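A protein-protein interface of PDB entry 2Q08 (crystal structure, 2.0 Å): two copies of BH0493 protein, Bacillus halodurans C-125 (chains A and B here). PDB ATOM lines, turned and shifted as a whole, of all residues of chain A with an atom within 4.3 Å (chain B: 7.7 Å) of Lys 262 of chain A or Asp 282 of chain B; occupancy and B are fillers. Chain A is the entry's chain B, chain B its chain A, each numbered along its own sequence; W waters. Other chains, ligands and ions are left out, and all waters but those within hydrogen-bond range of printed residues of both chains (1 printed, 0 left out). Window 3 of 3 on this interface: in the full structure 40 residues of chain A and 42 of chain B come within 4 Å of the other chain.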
ATOM      1  N   PRO A 226     -38.932 -18.888  32.472  1.00  0.00           N
ATOM      2  CA  PRO A 226     -38.539 -17.607  31.861  1.00  0.00           C
ATOM      3  C   PRO A 226     -39.571 -17.125  30.840  1.00  0.00           C
ATOM      4  O   PRO A 226     -39.735 -15.923  30.611  1.00  0.00           O
ATOM      5  CB  PRO A 226     -37.205 -17.935  31.191  1.00  0.00           C
ATOM      6  CG  PRO A 226     -36.644 -19.016  32.053  1.00  0.00           C
ATOM      7  CD  PRO A 226     -37.856 -19.890  32.344  1.00  0.00           C
ATOM      8  N   GLY A 260     -38.473 -17.510  36.567  1.00  0.00           N
ATOM      9  CA  GLY A 260     -37.181 -17.668  35.922  1.00  0.00           C
ATOM     10  C   GLY A 260     -36.519 -19.035  35.899  1.00  0.00           C
ATOM     11  O   GLY A 260     -35.442 -19.186  35.317  1.00  0.00           O
ATOM     12  N   VAL A 261     -37.149 -20.037  36.511  1.00  0.00           N
ATOM     13  CA  VAL A 261     -36.543 -21.359  36.545  1.00  0.00           C
ATOM     14  C   VAL A 261     -36.881 -22.192  35.312  1.00  0.00           C
ATOM     15  O   VAL A 261     -38.042 -22.318  34.938  1.00  0.00           O
ATOM     16  CB  VAL A 261     -36.951 -22.141  37.834  1.00  0.00           C
ATOM     17  CG1 VAL A 261     -38.462 -22.331  37.889  1.00  0.00           C
ATOM     18  CG2 VAL A 261     -36.242 -23.485  37.873  1.00  0.00           C
ATOM     19  N   LYS A 262     -35.849 -22.725  34.662  1.00  0.00           N
ATOM     20  CA  LYS A 262     -36.039 -23.576  33.489  1.00  0.00           C
ATOM     21  C   LYS A 262     -35.775 -24.997  34.008  1.00  0.00           C
ATOM     22  O   LYS A 262     -34.633 -25.383  34.252  1.00  0.00           O
ATOM     23  CB  LYS A 262     -35.041 -23.205  32.380  1.00  0.00           C
ATOM     24  CG  LYS A 262     -35.339 -23.894  31.046  1.00  0.00           C
ATOM     25  CD  LYS A 262     -34.414 -23.430  29.918  1.00  0.00           C
ATOM     26  CE  LYS A 262     -34.720 -24.191  28.626  1.00  0.00           C
ATOM     27  NZ  LYS A 262     -33.841 -23.797  27.490  1.00  0.00           N
ATOM     28  N   LYS A 263     -36.850 -25.755  34.190  1.00  0.00           N
ATOM     29  CA  LYS A 263     -36.775 -27.107  34.738  1.00  0.00           C
ATOM     30  C   LYS A 263     -36.101 -28.195  33.910  1.00  0.00           C
ATOM     31  O   LYS A 263     -36.261 -28.270  32.696  1.00  0.00           O
ATOM     32  CB  LYS A 263     -38.183 -27.601  35.095  1.00  0.00           C
ATOM     33  CG  LYS A 263     -38.980 -26.681  36.012  1.00  0.00           C
ATOM     34  CD  LYS A 263     -38.395 -26.623  37.416  1.00  0.00           C
ATOM     35  CE  LYS A 263     -38.548 -27.954  38.142  1.00  0.00           C
ATOM     36  NZ  LYS A 263     -37.961 -27.899  39.515  1.00  0.00           N
ATOM     37  N   ARG A 264     -35.342 -29.033  34.608  1.00  0.00           N
ATOM     38  CA  ARG A 264     -34.683 -30.194  34.024  1.00  0.00           C
ATOM     39  C   ARG A 264     -33.897 -30.047  32.728  1.00  0.00           C
ATOM     40  O   ARG A 264     -34.168 -30.775  31.775  1.00  0.00           O
ATOM     41  CB  ARG A 264     -35.727 -31.288  33.813  1.00  0.00           C
ATOM     42  CG  ARG A 264     -36.622 -31.554  35.012  1.00  0.00           C
ATOM     43  CD  ARG A 264     -37.908 -32.290  34.601  1.00  0.00           C
ATOM     44  NE  ARG A 264     -37.653 -33.516  33.838  1.00  0.00           N
ATOM     45  CZ  ARG A 264     -37.547 -33.579  32.509  1.00  0.00           C
ATOM     46  NH1 ARG A 264     -37.679 -32.482  31.771  1.00  0.00           N
ATOM     47  NH2 ARG A 264     -37.308 -34.745  31.915  1.00  0.00           N
ATOM     48  N   VAL A 265     -32.933 -29.135  32.666  1.00  0.00           N
ATOM     49  CA  VAL A 265     -32.142 -29.017  31.446  1.00  0.00           C
ATOM     50  C   VAL A 265     -31.143 -30.177  31.449  1.00  0.00           C
ATOM     51  O   VAL A 265     -30.587 -30.542  30.417  1.00  0.00           O
ATOM     52  CB  VAL A 265     -31.395 -27.662  31.362  1.00  0.00           C
ATOM     53  CG1 VAL A 265     -32.406 -26.522  31.423  1.00  0.00           C
ATOM     54  CG2 VAL A 265     -30.364 -27.554  32.463  1.00  0.00           C
ATOM     55  N   ASP A 274     -31.883 -27.995  37.273  1.00  0.00           N
ATOM     56  CA  ASP A 274     -32.658 -26.836  36.855  1.00  0.00           C
ATOM     57  C   ASP A 274     -31.751 -25.680  36.461  1.00  0.00           C
ATOM     58  O   ASP A 274     -30.732 -25.447  37.095  1.00  0.00           O
ATOM     59  CB  ASP A 274     -33.617 -26.403  37.965  1.00  0.00           C
ATOM     60  CG  ASP A 274     -34.694 -27.443  38.239  1.00  0.00           C
ATOM     61  OD1 ASP A 274     -34.926 -28.309  37.360  1.00  0.00           O
ATOM     62  OD2 ASP A 274     -35.318 -27.390  39.321  1.00  0.00           O
ATOM     63  N   PHE A 275     -32.157 -24.961  35.417  1.00  0.00           N
ATOM     64  CA  PHE A 275     -31.386 -23.840  34.875  1.00  0.00           C
ATOM     65  C   PHE A 275     -32.147 -22.529  35.079  1.00  0.00           C
ATOM     66  O   PHE A 275     -33.176 -22.508  35.754  1.00  0.00           O
ATOM     67  CB  PHE A 275     -31.124 -24.112  33.386  1.00  0.00           C
ATOM     68  CG  PHE A 275     -30.165 -23.159  32.735  1.00  0.00           C
ATOM     69  CD1 PHE A 275     -29.026 -22.717  33.405  1.00  0.00           C
ATOM     70  CD2 PHE A 275     -30.386 -22.732  31.420  1.00  0.00           C
ATOM     71  CE1 PHE A 275     -28.120 -21.863  32.780  1.00  0.00           C
ATOM     72  CE2 PHE A 275     -29.479 -21.876  30.788  1.00  0.00           C
ATOM     73  CZ  PHE A 275     -28.345 -21.442  31.471  1.00  0.00           C
ATOM     74  N   PHE B 228     -26.459 -16.983  17.459  1.00  0.00           N
ATOM     75  CA  PHE B 228     -26.122 -18.399  17.378  1.00  0.00           C
ATOM     76  C   PHE B 228     -27.197 -19.306  17.945  1.00  0.00           C
ATOM     77  O   PHE B 228     -27.698 -19.082  19.050  1.00  0.00           O
ATOM     78  CB  PHE B 228     -24.811 -18.689  18.111  1.00  0.00           C
ATOM     79  CG  PHE B 228     -24.459 -20.153  18.159  1.00  0.00           C
ATOM     80  CD1 PHE B 228     -24.126 -20.840  16.991  1.00  0.00           C
ATOM     81  CD2 PHE B 228     -24.483 -20.850  19.365  1.00  0.00           C
ATOM     82  CE1 PHE B 228     -23.819 -22.203  17.022  1.00  0.00           C
ATOM     83  CE2 PHE B 228     -24.176 -22.221  19.412  1.00  0.00           C
ATOM     84  CZ  PHE B 228     -23.844 -22.899  18.237  1.00  0.00           C
ATOM     85  N   SER B 229     -27.551 -20.339  17.190  1.00  0.00           N
ATOM     86  CA  SER B 229     -28.544 -21.301  17.649  1.00  0.00           C
ATOM     87  C   SER B 229     -28.173 -22.696  17.173  1.00  0.00           C
ATOM     88  O   SER B 229     -27.468 -22.862  16.177  1.00  0.00           O
ATOM     89  CB  SER B 229     -29.939 -20.924  17.147  1.00  0.00           C
ATOM     90  OG  SER B 229     -30.001 -20.989  15.739  1.00  0.00           O
ATOM     91  N   PHE B 230     -28.644 -23.698  17.903  1.00  0.00           N
ATOM     92  CA  PHE B 230     -28.374 -25.088  17.570  1.00  0.00           C
ATOM     93  C   PHE B 230     -29.357 -25.967  18.331  1.00  0.00           C
ATOM     94  O   PHE B 230     -29.589 -25.751  19.516  1.00  0.00           O
ATOM     95  CB  PHE B 230     -26.933 -25.454  17.948  1.00  0.00           C
ATOM     96  CG  PHE B 230     -26.549 -26.857  17.576  1.00  0.00           C
ATOM     97  CD1 PHE B 230     -26.976 -27.941  18.342  1.00  0.00           C
ATOM     98  CD2 PHE B 230     -25.797 -27.100  16.428  1.00  0.00           C
ATOM     99  CE1 PHE B 230     -26.663 -29.246  17.969  1.00  0.00           C
ATOM    100  CE2 PHE B 230     -25.476 -28.404  16.042  1.00  0.00           C
ATOM    101  CZ  PHE B 230     -25.910 -29.480  16.813  1.00  0.00           C
ATOM    102  N   PRO B 231     -29.946 -26.975  17.661  1.00  0.00           N
ATOM    103  CA  PRO B 231     -29.756 -27.347  16.253  1.00  0.00           C
ATOM    104  C   PRO B 231     -30.174 -26.241  15.291  1.00  0.00           C
ATOM    105  O   PRO B 231     -30.887 -25.311  15.664  1.00  0.00           O
ATOM    106  CB  PRO B 231     -30.635 -28.584  16.094  1.00  0.00           C
ATOM    107  CG  PRO B 231     -30.703 -29.152  17.483  1.00  0.00           C
ATOM    108  CD  PRO B 231     -30.862 -27.919  18.324  1.00  0.00           C
ATOM    109  N   ALA B 279     -26.524 -13.415  23.779  1.00  0.00           N
ATOM    110  CA  ALA B 279     -26.986 -14.580  23.032  1.00  0.00           C
ATOM    111  C   ALA B 279     -27.976 -15.407  23.858  1.00  0.00           C
ATOM    112  O   ALA B 279     -28.109 -15.213  25.070  1.00  0.00           O
ATOM    113  CB  ALA B 279     -25.795 -15.443  22.650  1.00  0.00           C
ATOM    114  N   SER B 280     -28.676 -16.315  23.192  1.00  0.00           N
ATOM    115  CA  SER B 280     -29.600 -17.210  23.895  1.00  0.00           C
ATOM    116  C   SER B 280     -28.694 -18.322  24.414  1.00  0.00           C
ATOM    117  O   SER B 280     -27.656 -18.590  23.812  1.00  0.00           O
ATOM    118  CB  SER B 280     -30.624 -17.806  22.923  1.00  0.00           C
ATOM    119  OG  SER B 280     -31.324 -18.881  23.524  1.00  0.00           O
ATOM    120  N   MET B 281     -29.064 -18.962  25.522  1.00  0.00           N
ATOM    121  CA  MET B 281     -28.251 -20.060  26.046  1.00  0.00           C
ATOM    122  C   MET B 281     -28.756 -21.409  25.509  1.00  0.00           C
ATOM    123  O   MET B 281     -28.119 -22.439  25.712  1.00  0.00           O
ATOM    124  CB  MET B 281     -28.293 -20.090  27.585  1.00  0.00           C
ATOM    125  CG  MET B 281     -27.781 -18.840  28.282  1.00  0.00           C
ATOM    126  SD  MET B 281     -26.088 -18.398  27.840  1.00  0.00           S
ATOM    127  CE  MET B 281     -25.190 -19.755  28.614  1.00  0.00           C
ATOM    128  N   ASP B 282     -29.895 -21.391  24.825  1.00  0.00           N
ATOM    129  CA  ASP B 282     -30.511 -22.616  24.294  1.00  0.00           C
ATOM    130  C   ASP B 282     -29.597 -23.533  23.479  1.00  0.00           C
ATOM    131  O   ASP B 282     -29.607 -24.747  23.662  1.00  0.00           O
ATOM    132  CB  ASP B 282     -31.737 -22.260  23.448  1.00  0.00           C
ATOM    133  CG  ASP B 282     -32.868 -21.669  24.273  1.00  0.00           C
ATOM    134  OD1 ASP B 282     -32.703 -21.524  25.501  1.00  0.00           O
ATOM    135  OD2 ASP B 282     -33.926 -21.348  23.698  1.00  0.00           O
ATOM    136  N   GLY B 283     -28.819 -22.947  22.576  1.00  0.00           N
ATOM    137  CA  GLY B 283     -27.932 -23.741  21.738  1.00  0.00           C
ATOM    138  C   GLY B 283     -26.842 -24.435  22.526  1.00  0.00           C
ATOM    139  O   GLY B 283     -26.561 -25.611  22.292  1.00  0.00           O
ATOM    140  N   VAL B 284     -26.224 -23.705  23.455  1.00  0.00           N
ATOM    141  CA  VAL B 284     -25.168 -24.265  24.285  1.00  0.00           C
ATOM    142  C   VAL B 284     -25.767 -25.339  25.193  1.00  0.00           C
ATOM    143  O   VAL B 284     -25.189 -26.408  25.376  1.00  0.00           O
ATOM    144  CB  VAL B 284     -24.504 -23.177  25.148  1.00  0.00           C
ATOM    145  CG1 VAL B 284     -23.356 -23.771  25.951  1.00  0.00           C
ATOM    146  CG2 VAL B 284     -24.001 -22.051  24.261  1.00  0.00           C
ATOM    147  N   GLU B 285     -26.934 -25.040  25.758  1.00  0.00           N
ATOM    148  CA  GLU B 285     -27.623 -25.979  26.631  1.00  0.00           C
ATOM    149  C   GLU B 285     -27.878 -27.292  25.878  1.00  0.00           C
ATOM    150  O   GLU B 285     -27.634 -28.384  26.393  1.00  0.00           O
ATOM    151  CB  GLU B 285     -28.956 -25.380  27.076  1.00  0.00           C
ATOM    152  CG  GLU B 285     -29.765 -26.266  28.010  1.00  0.00           C
ATOM    153  CD  GLU B 285     -31.222 -25.855  28.052  1.00  0.00           C
ATOM    154  OE1 GLU B 285     -31.479 -24.635  28.129  1.00  0.00           O
ATOM    155  OE2 GLU B 285     -32.106 -26.746  28.010  1.00  0.00           O
ATOM    156  N   HIS B 286     -28.372 -27.170  24.653  1.00  0.00           N
ATOM    157  CA  HIS B 286     -28.670 -28.341  23.838  1.00  0.00           C
ATOM    158  C   HIS B 286     -27.415 -29.158  23.538  1.00  0.00           C
ATOM    159  O   HIS B 286     -27.414 -30.381  23.670  1.00  0.00           O
ATOM    160  CB  HIS B 286     -29.353 -27.905  22.536  1.00  0.00           C
ATOM    161  CG  HIS B 286     -29.722 -29.043  21.639  1.00  0.00           C
ATOM    162  ND1 HIS B 286     -28.786 -29.763  20.925  1.00  0.00           N
ATOM    163  CD2 HIS B 286     -30.923 -29.601  21.354  1.00  0.00           C
ATOM    164  CE1 HIS B 286     -29.396 -30.715  20.241  1.00  0.00           C
ATOM    165  NE2 HIS B 286     -30.692 -30.639  20.484  1.00  0.00           N
ATOM    166  N   LEU B 287     -26.347 -28.481  23.135  1.00  0.00           N
ATOM    167  CA  LEU B 287     -25.089 -29.159  22.835  1.00  0.00           C
ATOM    168  C   LEU B 287     -24.559 -29.935  24.036  1.00  0.00           C
ATOM    169  O   LEU B 287     -24.150 -31.094  23.907  1.00  0.00           O
ATOM    170  CB  LEU B 287     -24.034 -28.145  22.384  1.00  0.00           C
ATOM    171  CG  LEU B 287     -24.212 -27.594  20.965  1.00  0.00           C
ATOM    172  CD1 LEU B 287     -23.336 -26.351  20.782  1.00  0.00           C
ATOM    173  CD2 LEU B 287     -23.852 -28.677  19.948  1.00  0.00           C
ATOM    174  N   LEU B 288     -24.569 -29.298  25.203  1.00  0.00           N
ATOM    175  CA  LEU B 288     -24.075 -29.941  26.420  1.00  0.00           C
ATOM    176  C   LEU B 288     -24.899 -31.162  26.805  1.00  0.00           C
ATOM    177  O   LEU B 288     -24.347 -32.199  27.157  1.00  0.00           O
ATOM    178  CB  LEU B 288     -24.076 -28.944  27.586  1.00  0.00           C
ATOM    179  CG  LEU B 288     -23.106 -27.769  27.439  1.00  0.00           C
ATOM    180  CD1 LEU B 288     -23.394 -26.725  28.513  1.00  0.00           C
ATOM    181  CD2 LEU B 288     -21.673 -28.277  27.546  1.00  0.00           C
ATOM    182  N   ARG B 289     -26.217 -31.029  26.746  1.00  0.00           N
ATOM    183  CA  ARG B 289     -27.105 -32.125  27.109  1.00  0.00           C
ATOM    184  C   ARG B 289     -27.129 -33.277  26.102  1.00  0.00           C
ATOM    185  O   ARG B 289     -27.059 -34.436  26.491  1.00  0.00           O
ATOM    186  CB  ARG B 289     -28.541 -31.617  27.298  1.00  0.00           C
ATOM    187  CG  ARG B 289     -29.533 -32.745  27.579  1.00  0.00           C
ATOM    188  CD  ARG B 289     -30.955 -32.252  27.774  1.00  0.00           C
ATOM    189  NE  ARG B 289     -31.396 -31.411  26.671  1.00  0.00           N
ATOM    190  CZ  ARG B 289     -31.570 -30.094  26.760  1.00  0.00           C
ATOM    191  NH1 ARG B 289     -31.346 -29.465  27.912  1.00  0.00           N
ATOM    192  NH2 ARG B 289     -31.957 -29.405  25.697  1.00  0.00           N
ATOM    193  N   GLU B 308     -25.758 -16.372  33.852  1.00  0.00           N
ATOM    194  CA  GLU B 308     -26.430 -17.597  33.402  1.00  0.00           C
ATOM    195  C   GLU B 308     -25.442 -18.623  32.849  1.00  0.00           C
ATOM    196  O   GLU B 308     -25.709 -19.821  32.894  1.00  0.00           O
ATOM    197  CB  GLU B 308     -27.538 -17.292  32.375  1.00  0.00           C
ATOM    198  CG  GLU B 308     -27.104 -16.520  31.154  1.00  0.00           C
ATOM    199  CD  GLU B 308     -28.275 -15.965  30.370  1.00  0.00           C
ATOM    200  OE1 GLU B 308     -29.409 -15.992  30.896  1.00  0.00           O
ATOM    201  OE2 GLU B 308     -28.063 -15.490  29.226  1.00  0.00           O
ATOM    202  N   LEU B 312     -25.108 -22.425  33.968  1.00  0.00           N
ATOM    203  CA  LEU B 312     -25.090 -23.545  33.029  1.00  0.00           C
ATOM    204  C   LEU B 312     -23.944 -24.499  33.369  1.00  0.00           C
ATOM    205  O   LEU B 312     -24.079 -25.718  33.232  1.00  0.00           O
ATOM    206  CB  LEU B 312     -24.954 -23.047  31.590  1.00  0.00           C
ATOM    207  CG  LEU B 312     -25.184 -24.109  30.502  1.00  0.00           C
ATOM    208  CD1 LEU B 312     -26.528 -24.783  30.706  1.00  0.00           C
ATOM    209  CD2 LEU B 312     -25.123 -23.459  29.128  1.00  0.00           C
ATOM    210  N   LYS B 315     -24.752 -27.001  35.847  1.00  0.00           N
ATOM    211  CA  LYS B 315     -25.577 -28.071  35.290  1.00  0.00           C
ATOM    212  C   LYS B 315     -24.829 -29.140  34.497  1.00  0.00           C
ATOM    213  O   LYS B 315     -25.231 -30.293  34.504  1.00  0.00           O
ATOM    214  CB  LYS B 315     -26.653 -27.490  34.360  1.00  0.00           C
ATOM    215  CG  LYS B 315     -27.555 -26.412  34.946  1.00  0.00           C
ATOM    216  CD  LYS B 315     -28.576 -26.970  35.909  1.00  0.00           C
ATOM    217  CE  LYS B 315     -28.058 -26.988  37.338  1.00  0.00           C
ATOM    218  NZ  LYS B 315     -27.753 -25.635  37.821  1.00  0.00           N
HETATM  219  O   HOH W   1     -31.384 -22.132  27.897  1.00  0.00           O
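Lys 262 of chain A touches just these residues of chain B: Asp 282 (3.2 Å) and Glu 285 (2.6 Å).
Of chain A, only Lys 262 (3.2 Å) comes within 4 Å of Asp 282 of chain B.
Of the printed residues of chain A, Glu 308 of chain B touches Phe 275 (3.2 Å).
Of the printed residues of chain A, Lys 315 of chain B touches Val 265 and Asp 274.
Printed residues of chain A within 4 Å of Arg 289 of chain B: Val 265.
Of the printed residues of chain B, Phe 275 of chain A touches Met 281 (3.9 Å), Glu 285 (3.96 Å), Glu 308 (3.2 Å) and Leu 312 (3.3 Å).
The nearest printed residue of chain A that does not touch Asp 282 of chain B is Phe 275 of chain A (6.0 Å).
Hydrophobic or aromatic side chains of chain A within 4 Å of the printed part of chain B: Val 265 and Phe 275.
Among the printed residues, 10 pairs touch across the chains.
Among the printed residues, Asp or Glu carboxylates within 4 Å of a Lys or Arg side-chain nitrogen of the other chain: Lys 262 of chain A with Asp 282 of chain B (3.2 Å) and Lys 262 of chain A with Glu 285 of chain B (2.6 Å).
Water W1 lies within hydrogen-bond range of the side-chain carboxylate (OE1) of Glu 285 of chain B, the side-chain carboxylate (OD1) of Asp 282 of chain B and the side-chain amino group (NZ) of Lys 262 of chain A.
Among the printed residues, merely in contact across the chains: Val 265 of chain A with Glu 285 of chain B, Val 265 of chain A with Lys 315 of chain B, Phe 275 of chain A with Met 281 of chain B, Phe 275 of chain A with Glu 285 of chain B, Phe 275 of chain A with Glu 308 of chain B and Phe 275 of chain A with Leu 312 of chain B.
The side-chain amino group (NZ) of Lys 263 of chain A is in salt-bridge range of the side-chain carboxylate (OD2) of Asp 274 of chain A (2.7 Å).
The backbone NH (N) of Arg 264 of chain A is in hydrogen-bond range of the side-chain carboxylate (OD1) of Asp 274 of chain A.
O of Lys 262 of chain A lies within hydrogen-bond range of N of Phe 275 of chain A, at 2.8 Å.
The guanidinium group of Arg 289 of chain B is in salt-bridge range of the side-chain carboxylate of Glu 285 of chain B (2.8 Å).
The side-chain hydroxyl (OG) of Ser 280 of chain B lies within hydrogen-bond range of the backbone NH (N) of Asp 282 of chain B (3.2 Å).
The side-chain amino group of Lys 315 of chain B lies close to the backbone carbonyl oxygen of Asp 274 of chain A, at 3.1 Å.
The guanidinium group (NH1) of Arg 289 of chain B is in hydrogen-bond range of the backbone carbonyl oxygen (O) of Val 265 of chain A, at 2.8 Å.
NZ of Lys 262 of chain A lies within salt-bridge range of OD1 of Asp 282 of chain B (3.2 Å).
The side-chain carboxylate of Glu 285 of chain B is in salt-bridge range of the side-chain amino group of Lys 262 of chain A, at 2.6 Å.
No position is printed for both chains.
Of the 10 pairs that touch across the chains among the printed residues, none has its exchanged pair printed and touching as well.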
